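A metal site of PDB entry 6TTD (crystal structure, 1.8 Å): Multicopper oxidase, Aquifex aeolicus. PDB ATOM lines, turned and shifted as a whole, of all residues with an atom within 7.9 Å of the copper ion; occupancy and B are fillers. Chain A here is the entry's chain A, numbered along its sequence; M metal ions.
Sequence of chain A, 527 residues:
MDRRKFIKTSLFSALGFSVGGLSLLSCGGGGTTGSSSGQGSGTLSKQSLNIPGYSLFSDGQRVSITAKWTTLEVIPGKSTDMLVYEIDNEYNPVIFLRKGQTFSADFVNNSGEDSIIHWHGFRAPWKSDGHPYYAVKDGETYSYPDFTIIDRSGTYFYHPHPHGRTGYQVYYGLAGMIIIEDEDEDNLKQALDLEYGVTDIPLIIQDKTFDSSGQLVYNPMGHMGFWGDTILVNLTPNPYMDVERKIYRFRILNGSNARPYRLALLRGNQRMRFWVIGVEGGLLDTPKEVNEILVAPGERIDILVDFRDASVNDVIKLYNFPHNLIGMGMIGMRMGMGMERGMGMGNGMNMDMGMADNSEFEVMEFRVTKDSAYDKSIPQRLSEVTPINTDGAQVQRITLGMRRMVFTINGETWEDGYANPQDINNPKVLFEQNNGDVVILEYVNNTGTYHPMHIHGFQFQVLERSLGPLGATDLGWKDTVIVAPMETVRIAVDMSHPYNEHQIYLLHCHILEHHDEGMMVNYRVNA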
ATOM      1  N   HIS A 223      11.215 -19.078 -25.147  1.00  0.00           N
ATOM      2  CA  HIS A 223      12.052 -18.187 -25.939  1.00  0.00           C
ATOM      3  C   HIS A 223      13.225 -17.614 -25.154  1.00  0.00           C
ATOM      4  O   HIS A 223      13.790 -16.590 -25.547  1.00  0.00           O
ATOM      5  CB  HIS A 223      11.163 -17.134 -26.597  1.00  0.00           C
ATOM      6  CG  HIS A 223      10.232 -17.746 -27.616  1.00  0.00           C
ATOM      7  ND1 HIS A 223      10.711 -18.377 -28.754  1.00  0.00           N
ATOM      8  CD2 HIS A 223       8.886 -17.886 -27.632  1.00  0.00           C
ATOM      9  CE1 HIS A 223       9.692 -18.865 -29.440  1.00  0.00           C
ATOM     10  NE2 HIS A 223       8.574 -18.583 -28.787  1.00  0.00           N
ATOM     11  N   MET A 224      13.532 -18.196 -24.000  1.00  0.00           N
ATOM     12  CA  MET A 224      14.704 -17.812 -23.227  1.00  0.00           C
ATOM     13  C   MET A 224      15.895 -18.705 -23.525  1.00  0.00           C
ATOM     14  O   MET A 224      16.900 -18.585 -22.831  1.00  0.00           O
ATOM     15  CB  MET A 224      14.441 -17.878 -21.717  1.00  0.00           C
ATOM     16  CG  MET A 224      13.207 -17.114 -21.260  1.00  0.00           C
ATOM     17  SD  MET A 224      13.335 -15.433 -21.831  1.00  0.00           S
ATOM     18  CE  MET A 224      12.195 -15.525 -23.209  1.00  0.00           C
ATOM     19  N   GLY A 225      15.822 -19.584 -24.521  1.00  0.00           N
ATOM     20  CA  GLY A 225      16.889 -20.532 -24.771  1.00  0.00           C
ATOM     21  C   GLY A 225      16.863 -21.681 -23.768  1.00  0.00           C
ATOM     22  O   GLY A 225      15.955 -21.819 -22.927  1.00  0.00           O
ATOM     23  N   LEU A 400      16.308  -4.792 -31.881  1.00  0.00           N
ATOM     24  CA  LEU A 400      15.914  -6.152 -31.496  1.00  0.00           C
ATOM     25  C   LEU A 400      14.444  -6.149 -31.121  1.00  0.00           C
ATOM     26  O   LEU A 400      14.023  -5.382 -30.239  1.00  0.00           O
ATOM     27  CB  LEU A 400      16.766  -6.662 -30.337  1.00  0.00           C
ATOM     28  CG  LEU A 400      18.274  -6.335 -30.454  1.00  0.00           C
ATOM     29  CD1 LEU A 400      19.050  -6.847 -29.214  1.00  0.00           C
ATOM     30  CD2 LEU A 400      18.845  -6.912 -31.720  1.00  0.00           C
ATOM     31  N   PHE A 407      12.279 -13.786 -32.301  1.00  0.00           N
ATOM     32  CA  PHE A 407      13.070 -12.563 -32.165  1.00  0.00           C
ATOM     33  C   PHE A 407      13.512 -12.079 -33.544  1.00  0.00           C
ATOM     34  O   PHE A 407      13.726 -12.889 -34.473  1.00  0.00           O
ATOM     35  CB  PHE A 407      14.271 -12.772 -31.220  1.00  0.00           C
ATOM     36  CG  PHE A 407      13.862 -12.983 -29.790  1.00  0.00           C
ATOM     37  CD1 PHE A 407      13.259 -11.945 -29.070  1.00  0.00           C
ATOM     38  CD2 PHE A 407      14.035 -14.198 -29.172  1.00  0.00           C
ATOM     39  CE1 PHE A 407      12.856 -12.116 -27.743  1.00  0.00           C
ATOM     40  CE2 PHE A 407      13.627 -14.383 -27.837  1.00  0.00           C
ATOM     41  CZ  PHE A 407      13.033 -13.352 -27.125  1.00  0.00           C
ATOM     42  N   ASN A 445      17.272  -2.788 -27.672  1.00  0.00           N
ATOM     43  CA  ASN A 445      16.563  -4.005 -27.295  1.00  0.00           C
ATOM     44  C   ASN A 445      15.106  -3.687 -26.901  1.00  0.00           C
ATOM     45  O   ASN A 445      14.814  -3.322 -25.752  1.00  0.00           O
ATOM     46  CB  ASN A 445      17.312  -4.704 -26.159  1.00  0.00           C
ATOM     47  CG  ASN A 445      16.705  -6.047 -25.808  1.00  0.00           C
ATOM     48  OD1 ASN A 445      15.721  -6.483 -26.432  1.00  0.00           O
ATOM     49  ND2 ASN A 445      17.357  -6.760 -24.865  1.00  0.00           N
ATOM     50  N   THR A 447      12.780  -5.786 -26.402  1.00  0.00           N
ATOM     51  CA  THR A 447      12.197  -7.040 -25.947  1.00  0.00           C
ATOM     52  C   THR A 447      12.451  -7.166 -24.456  1.00  0.00           C
ATOM     53  O   THR A 447      13.216  -6.393 -23.860  1.00  0.00           O
ATOM     54  CB  THR A 447      12.777  -8.241 -26.693  1.00  0.00           C
ATOM     55  OG1 THR A 447      14.043  -8.591 -26.123  1.00  0.00           O
ATOM     56  CG2 THR A 447      12.924  -7.912 -28.202  1.00  0.00           C
ATOM     57  N   THR A 449      13.888  -9.661 -22.813  1.00  0.00           N
ATOM     58  CA  THR A 449      14.936 -10.551 -22.367  1.00  0.00           C
ATOM     59  C   THR A 449      16.252 -10.034 -22.930  1.00  0.00           C
ATOM     60  O   THR A 449      16.263  -9.353 -23.950  1.00  0.00           O
ATOM     61  CB  THR A 449      14.671 -11.975 -22.790  1.00  0.00           C
ATOM     62  OG1 THR A 449      15.759 -12.761 -22.301  1.00  0.00           O
ATOM     63  CG2 THR A 449      14.633 -12.076 -24.315  1.00  0.00           C
ATOM     64  N   TYR A 450      17.355 -10.344 -22.256  1.00  0.00           N
ATOM     65  CA  TYR A 450      18.645  -9.860 -22.737  1.00  0.00           C
ATOM     66  C   TYR A 450      19.083 -10.621 -23.987  1.00  0.00           C
ATOM     67  O   TYR A 450      18.613 -11.756 -24.263  1.00  0.00           O
ATOM     68  CB  TYR A 450      19.693 -10.012 -21.652  1.00  0.00           C
ATOM     69  CG  TYR A 450      20.438 -11.372 -21.649  1.00  0.00           C
ATOM     70  CD1 TYR A 450      21.740 -11.450 -22.067  1.00  0.00           C
ATOM     71  CD2 TYR A 450      19.830 -12.535 -21.183  1.00  0.00           C
ATOM     72  CE1 TYR A 450      22.459 -12.637 -22.045  1.00  0.00           C
ATOM     73  CE2 TYR A 450      20.524 -13.738 -21.121  1.00  0.00           C
ATOM     74  CZ  TYR A 450      21.859 -13.770 -21.571  1.00  0.00           C
ATOM     75  OH  TYR A 450      22.635 -14.911 -21.548  1.00  0.00           O
ATOM     76  N   HIS A 451      19.982  -9.970 -24.793  1.00  0.00           N
ATOM     77  CA  HIS A 451      20.574 -10.647 -25.943  1.00  0.00           C
ATOM     78  C   HIS A 451      22.067 -10.343 -25.945  1.00  0.00           C
ATOM     79  O   HIS A 451      22.443  -9.161 -25.992  1.00  0.00           O
ATOM     80  CB  HIS A 451      19.935 -10.197 -27.283  1.00  0.00           C
ATOM     81  CG  HIS A 451      18.449 -10.406 -27.330  1.00  0.00           C
ATOM     82  ND1 HIS A 451      17.889 -11.622 -27.653  1.00  0.00           N
ATOM     83  CD2 HIS A 451      17.421  -9.579 -27.039  1.00  0.00           C
ATOM     84  CE1 HIS A 451      16.570 -11.530 -27.572  1.00  0.00           C
ATOM     85  NE2 HIS A 451      16.261 -10.300 -27.175  1.00  0.00           N
ATOM     86  N   PRO A 452      22.938 -11.353 -25.893  1.00  0.00           N
ATOM     87  CA  PRO A 452      24.375 -11.078 -26.020  1.00  0.00           C
ATOM     88  C   PRO A 452      24.743 -11.006 -27.483  1.00  0.00           C
ATOM     89  O   PRO A 452      24.783 -12.066 -28.146  1.00  0.00           O
ATOM     90  CB  PRO A 452      25.028 -12.251 -25.274  1.00  0.00           C
ATOM     91  CG  PRO A 452      24.031 -13.436 -25.415  1.00  0.00           C
ATOM     92  CD  PRO A 452      22.632 -12.792 -25.626  1.00  0.00           C
ATOM     93  N   MET A 453      24.871  -9.777 -28.026  1.00  0.00           N
ATOM     94  CA  MET A 453      25.011  -9.559 -29.468  1.00  0.00           C
ATOM     95  C   MET A 453      26.488  -9.622 -29.881  1.00  0.00           C
ATOM     96  O   MET A 453      27.329  -8.892 -29.335  1.00  0.00           O
ATOM     97  CB  MET A 453      24.403  -8.224 -29.941  1.00  0.00           C
ATOM     98  CG  MET A 453      22.922  -8.166 -29.680  1.00  0.00           C
ATOM     99  SD  MET A 453      21.955  -9.510 -30.456  1.00  0.00           S
ATOM    100  CE  MET A 453      22.156  -9.104 -32.206  1.00  0.00           C
ATOM    101  N   VAL A 483      23.102  -6.916 -24.092  1.00  0.00           N
ATOM    102  CA  VAL A 483      22.108  -5.853 -24.265  1.00  0.00           C
ATOM    103  C   VAL A 483      20.901  -6.268 -23.459  1.00  0.00           C
ATOM    104  O   VAL A 483      20.106  -7.107 -23.915  1.00  0.00           O
ATOM    105  CB  VAL A 483      21.726  -5.644 -25.734  1.00  0.00           C
ATOM    106  CG1 VAL A 483      20.816  -4.349 -25.941  1.00  0.00           C
ATOM    107  CG2 VAL A 483      22.992  -5.583 -26.619  1.00  0.00           C
ATOM    108  N   HIS A 508      24.825 -11.528 -34.869  1.00  0.00           N
ATOM    109  CA  HIS A 508      23.734 -12.343 -34.349  1.00  0.00           C
ATOM    110  C   HIS A 508      23.770 -12.403 -32.826  1.00  0.00           C
ATOM    111  O   HIS A 508      24.739 -12.001 -32.172  1.00  0.00           O
ATOM    112  CB  HIS A 508      23.791 -13.778 -34.904  1.00  0.00           C
ATOM    113  CG  HIS A 508      24.989 -14.580 -34.448  1.00  0.00           C
ATOM    114  ND1 HIS A 508      25.022 -15.297 -33.252  1.00  0.00           N
ATOM    115  CD2 HIS A 508      26.168 -14.839 -35.074  1.00  0.00           C
ATOM    116  CE1 HIS A 508      26.185 -15.925 -33.158  1.00  0.00           C
ATOM    117  NE2 HIS A 508      26.897 -15.683 -34.252  1.00  0.00           N
ATOM    118  N   CYS A 509      22.673 -12.896 -32.275  1.00  0.00           N
ATOM    119  CA  CYS A 509      22.588 -13.139 -30.845  1.00  0.00           C
ATOM    120  C   CYS A 509      23.333 -14.420 -30.497  1.00  0.00           C
ATOM    121  O   CYS A 509      23.301 -15.415 -31.253  1.00  0.00           O
ATOM    122  CB  CYS A 509      21.112 -13.231 -30.422  1.00  0.00           C
ATOM    123  SG  CYS A 509      20.942 -13.507 -28.696  1.00  0.00           S
ATOM    124  N   HIS A 510      24.026 -14.406 -29.347  1.00  0.00           N
ATOM    125  CA  HIS A 510      24.744 -15.603 -28.944  1.00  0.00           C
ATOM    126  C   HIS A 510      23.995 -16.437 -27.903  1.00  0.00           C
ATOM    127  O   HIS A 510      24.574 -17.352 -27.328  1.00  0.00           O
ATOM    128  CB  HIS A 510      26.130 -15.243 -28.443  1.00  0.00           C
ATOM    129  CG  HIS A 510      27.136 -16.324 -28.691  1.00  0.00           C
ATOM    130  ND1 HIS A 510      27.167 -17.489 -27.965  1.00  0.00           N
ATOM    131  CD2 HIS A 510      28.150 -16.414 -29.596  1.00  0.00           C
ATOM    132  CE1 HIS A 510      28.170 -18.242 -28.391  1.00  0.00           C
ATOM    133  NE2 HIS A 510      28.784 -17.607 -29.374  1.00  0.00           N
ATOM    134  N   ILE A 511      22.714 -16.159 -27.665  1.00  0.00           N
ATOM    135  CA  ILE A 511      21.870 -17.197 -27.100  1.00  0.00           C
ATOM    136  C   ILE A 511      21.629 -18.195 -28.248  1.00  0.00           C
ATOM    137  O   ILE A 511      21.031 -17.843 -29.282  1.00  0.00           O
ATOM    138  CB  ILE A 511      20.581 -16.607 -26.507  1.00  0.00           C
ATOM    139  CG1 ILE A 511      20.971 -15.736 -25.266  1.00  0.00           C
ATOM    140  CG2 ILE A 511      19.591 -17.763 -26.093  1.00  0.00           C
ATOM    141  CD1 ILE A 511      19.859 -14.853 -24.774  1.00  0.00           C
ATOM    142  N   LEU A 512      22.170 -19.404 -28.105  1.00  0.00           N
ATOM    143  CA  LEU A 512      22.237 -20.313 -29.259  1.00  0.00           C
ATOM    144  C   LEU A 512      20.840 -20.726 -29.787  1.00  0.00           C
ATOM    145  O   LEU A 512      20.673 -20.897 -31.009  1.00  0.00           O
ATOM    146  CB  LEU A 512      23.080 -21.536 -28.913  1.00  0.00           C
ATOM    147  CG  LEU A 512      24.532 -21.237 -28.524  1.00  0.00           C
ATOM    148  CD1 LEU A 512      25.328 -22.586 -28.354  1.00  0.00           C
ATOM    149  CD2 LEU A 512      25.243 -20.310 -29.477  1.00  0.00           C
ATOM    150  N   GLU A 513      19.828 -20.863 -28.933  1.00  0.00           N
ATOM    151  CA  GLU A 513      18.459 -21.091 -29.438  1.00  0.00           C
ATOM    152  C   GLU A 513      17.929 -19.880 -30.216  1.00  0.00           C
ATOM    153  O   GLU A 513      17.187 -20.046 -31.203  1.00  0.00           O
ATOM    154  CB  GLU A 513      17.513 -21.417 -28.289  1.00  0.00           C
ATOM    155  CG  GLU A 513      17.710 -22.850 -27.660  1.00  0.00           C
ATOM    156  CD  GLU A 513      19.045 -23.011 -26.935  1.00  0.00           C
ATOM    157  OE1 GLU A 513      19.507 -22.043 -26.262  1.00  0.00           O
ATOM    158  OE2 GLU A 513      19.662 -24.107 -27.041  1.00  0.00           O
ATOM    159  N   HIS A 514      18.296 -18.637 -29.816  1.00  0.00           N
ATOM    160  CA  HIS A 514      17.916 -17.473 -30.623  1.00  0.00           C
ATOM    161  C   HIS A 514      18.609 -17.515 -31.956  1.00  0.00           C
ATOM    162  O   HIS A 514      17.992 -17.319 -33.004  1.00  0.00           O
ATOM    163  CB  HIS A 514      18.277 -16.172 -29.907  1.00  0.00           C
ATOM    164  CG  HIS A 514      17.505 -15.977 -28.643  1.00  0.00           C
ATOM    165  ND1 HIS A 514      17.604 -14.838 -27.866  1.00  0.00           N
ATOM    166  CD2 HIS A 514      16.618 -16.782 -28.018  1.00  0.00           C
ATOM    167  CE1 HIS A 514      16.814 -14.953 -26.827  1.00  0.00           C
ATOM    168  NE2 HIS A 514      16.206 -16.123 -26.889  1.00  0.00           N
ATOM    169  N   HIS A 515      19.924 -17.749 -31.948  1.00  0.00           N
ATOM    170  CA  HIS A 515      20.651 -17.972 -33.201  1.00  0.00           C
ATOM    171  C   HIS A 515      19.936 -19.018 -34.052  1.00  0.00           C
ATOM    172  O   HIS A 515      19.621 -18.764 -35.221  1.00  0.00           O
ATOM    173  CB  HIS A 515      22.110 -18.402 -32.926  1.00  0.00           C
ATOM    174  CG  HIS A 515      22.798 -18.983 -34.120  1.00  0.00           C
ATOM    175  ND1 HIS A 515      22.603 -20.290 -34.532  1.00  0.00           N
ATOM    176  CD2 HIS A 515      23.650 -18.438 -35.015  1.00  0.00           C
ATOM    177  CE1 HIS A 515      23.307 -20.522 -35.626  1.00  0.00           C
ATOM    178  NE2 HIS A 515      23.951 -19.407 -35.940  1.00  0.00           N
ATOM    179  N   GLU A 517      16.928 -19.958 -34.104  1.00  0.00           N
ATOM    180  CA  GLU A 517      15.617 -19.564 -34.601  1.00  0.00           C
ATOM    181  C   GLU A 517      15.711 -18.461 -35.620  1.00  0.00           C
ATOM    182  O   GLU A 517      14.674 -17.977 -36.072  1.00  0.00           O
ATOM    183  CB  GLU A 517      14.697 -19.106 -33.473  1.00  0.00           C
ATOM    184  CG  GLU A 517      14.261 -20.244 -32.589  1.00  0.00           C
ATOM    185  CD  GLU A 517      13.851 -19.803 -31.204  1.00  0.00           C
ATOM    186  OE1 GLU A 517      13.637 -20.711 -30.337  1.00  0.00           O
ATOM    187  OE2 GLU A 517      13.784 -18.567 -30.965  1.00  0.00           O
ATOM    188  N   MET A 519      17.807 -15.440 -35.232  1.00  0.00           N
ATOM    189  CA  MET A 519      18.175 -14.089 -34.804  1.00  0.00           C
ATOM    190  C   MET A 519      19.610 -13.766 -35.273  1.00  0.00           C
ATOM    191  O   MET A 519      20.562 -13.658 -34.501  1.00  0.00           O
ATOM    192  CB  MET A 519      18.031 -13.988 -33.298  1.00  0.00           C
ATOM    193  CG  MET A 519      18.060 -12.548 -32.829  1.00  0.00           C
ATOM    194  SD  MET A 519      17.691 -12.358 -31.103  1.00  0.00           S
ATOM    195  CE  MET A 519      17.801 -10.539 -31.043  1.00  0.00           C
HETATM  196 CU    CU M   1      18.840 -13.318 -28.200  1.00  0.00          CU
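The copper ion is bound by a ring nitrogen (ND1) of His 514, a ring nitrogen (ND1) of His 451 and the side-chain sulfur (SG) of Cys 509.
Merely in contact with the copper ion: Ile 511 (3.9 Å) and Met 519 (3.3 Å).
Five residues have an atom within 4 Å of the copper ion: His 451, Cys 509, Ile 511, His 514 and Met 519.
The backbone NH (N) of Met 519 is in hydrogen-bond range of the backbone carbonyl oxygen (O) of His 514, 2.9 Å away.
O of His 223 lies within hydrogen-bond range of NE2 of His 514 (2.8 Å).
The side-chain sulfur of Met 519 sits close to a ring nitrogen (ND1) of His 451.
A ring nitrogen (NE2) of His 451 lies close to the backbone carbonyl oxygen (O) of Thr 449 (3.4 Å).
The side-chain hydroxyl (OG1) of Thr 447 lies within hydrogen-bond range of a ring nitrogen (NE2) of His 451 (3.0 Å).
The backbone NH (N) of His 451 is in hydrogen-bond range of the backbone carbonyl oxygen (O) of Val 483 (3.0 Å).
The backbone NH (N) of Cys 509 is in hydrogen-bond range of the backbone carbonyl oxygen (O) of Met 519, at 3.2 Å.
The side-chain sulfur (SG) of Cys 509 lies close to the backbone NH (N) of Ile 511 (3.4 Å).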
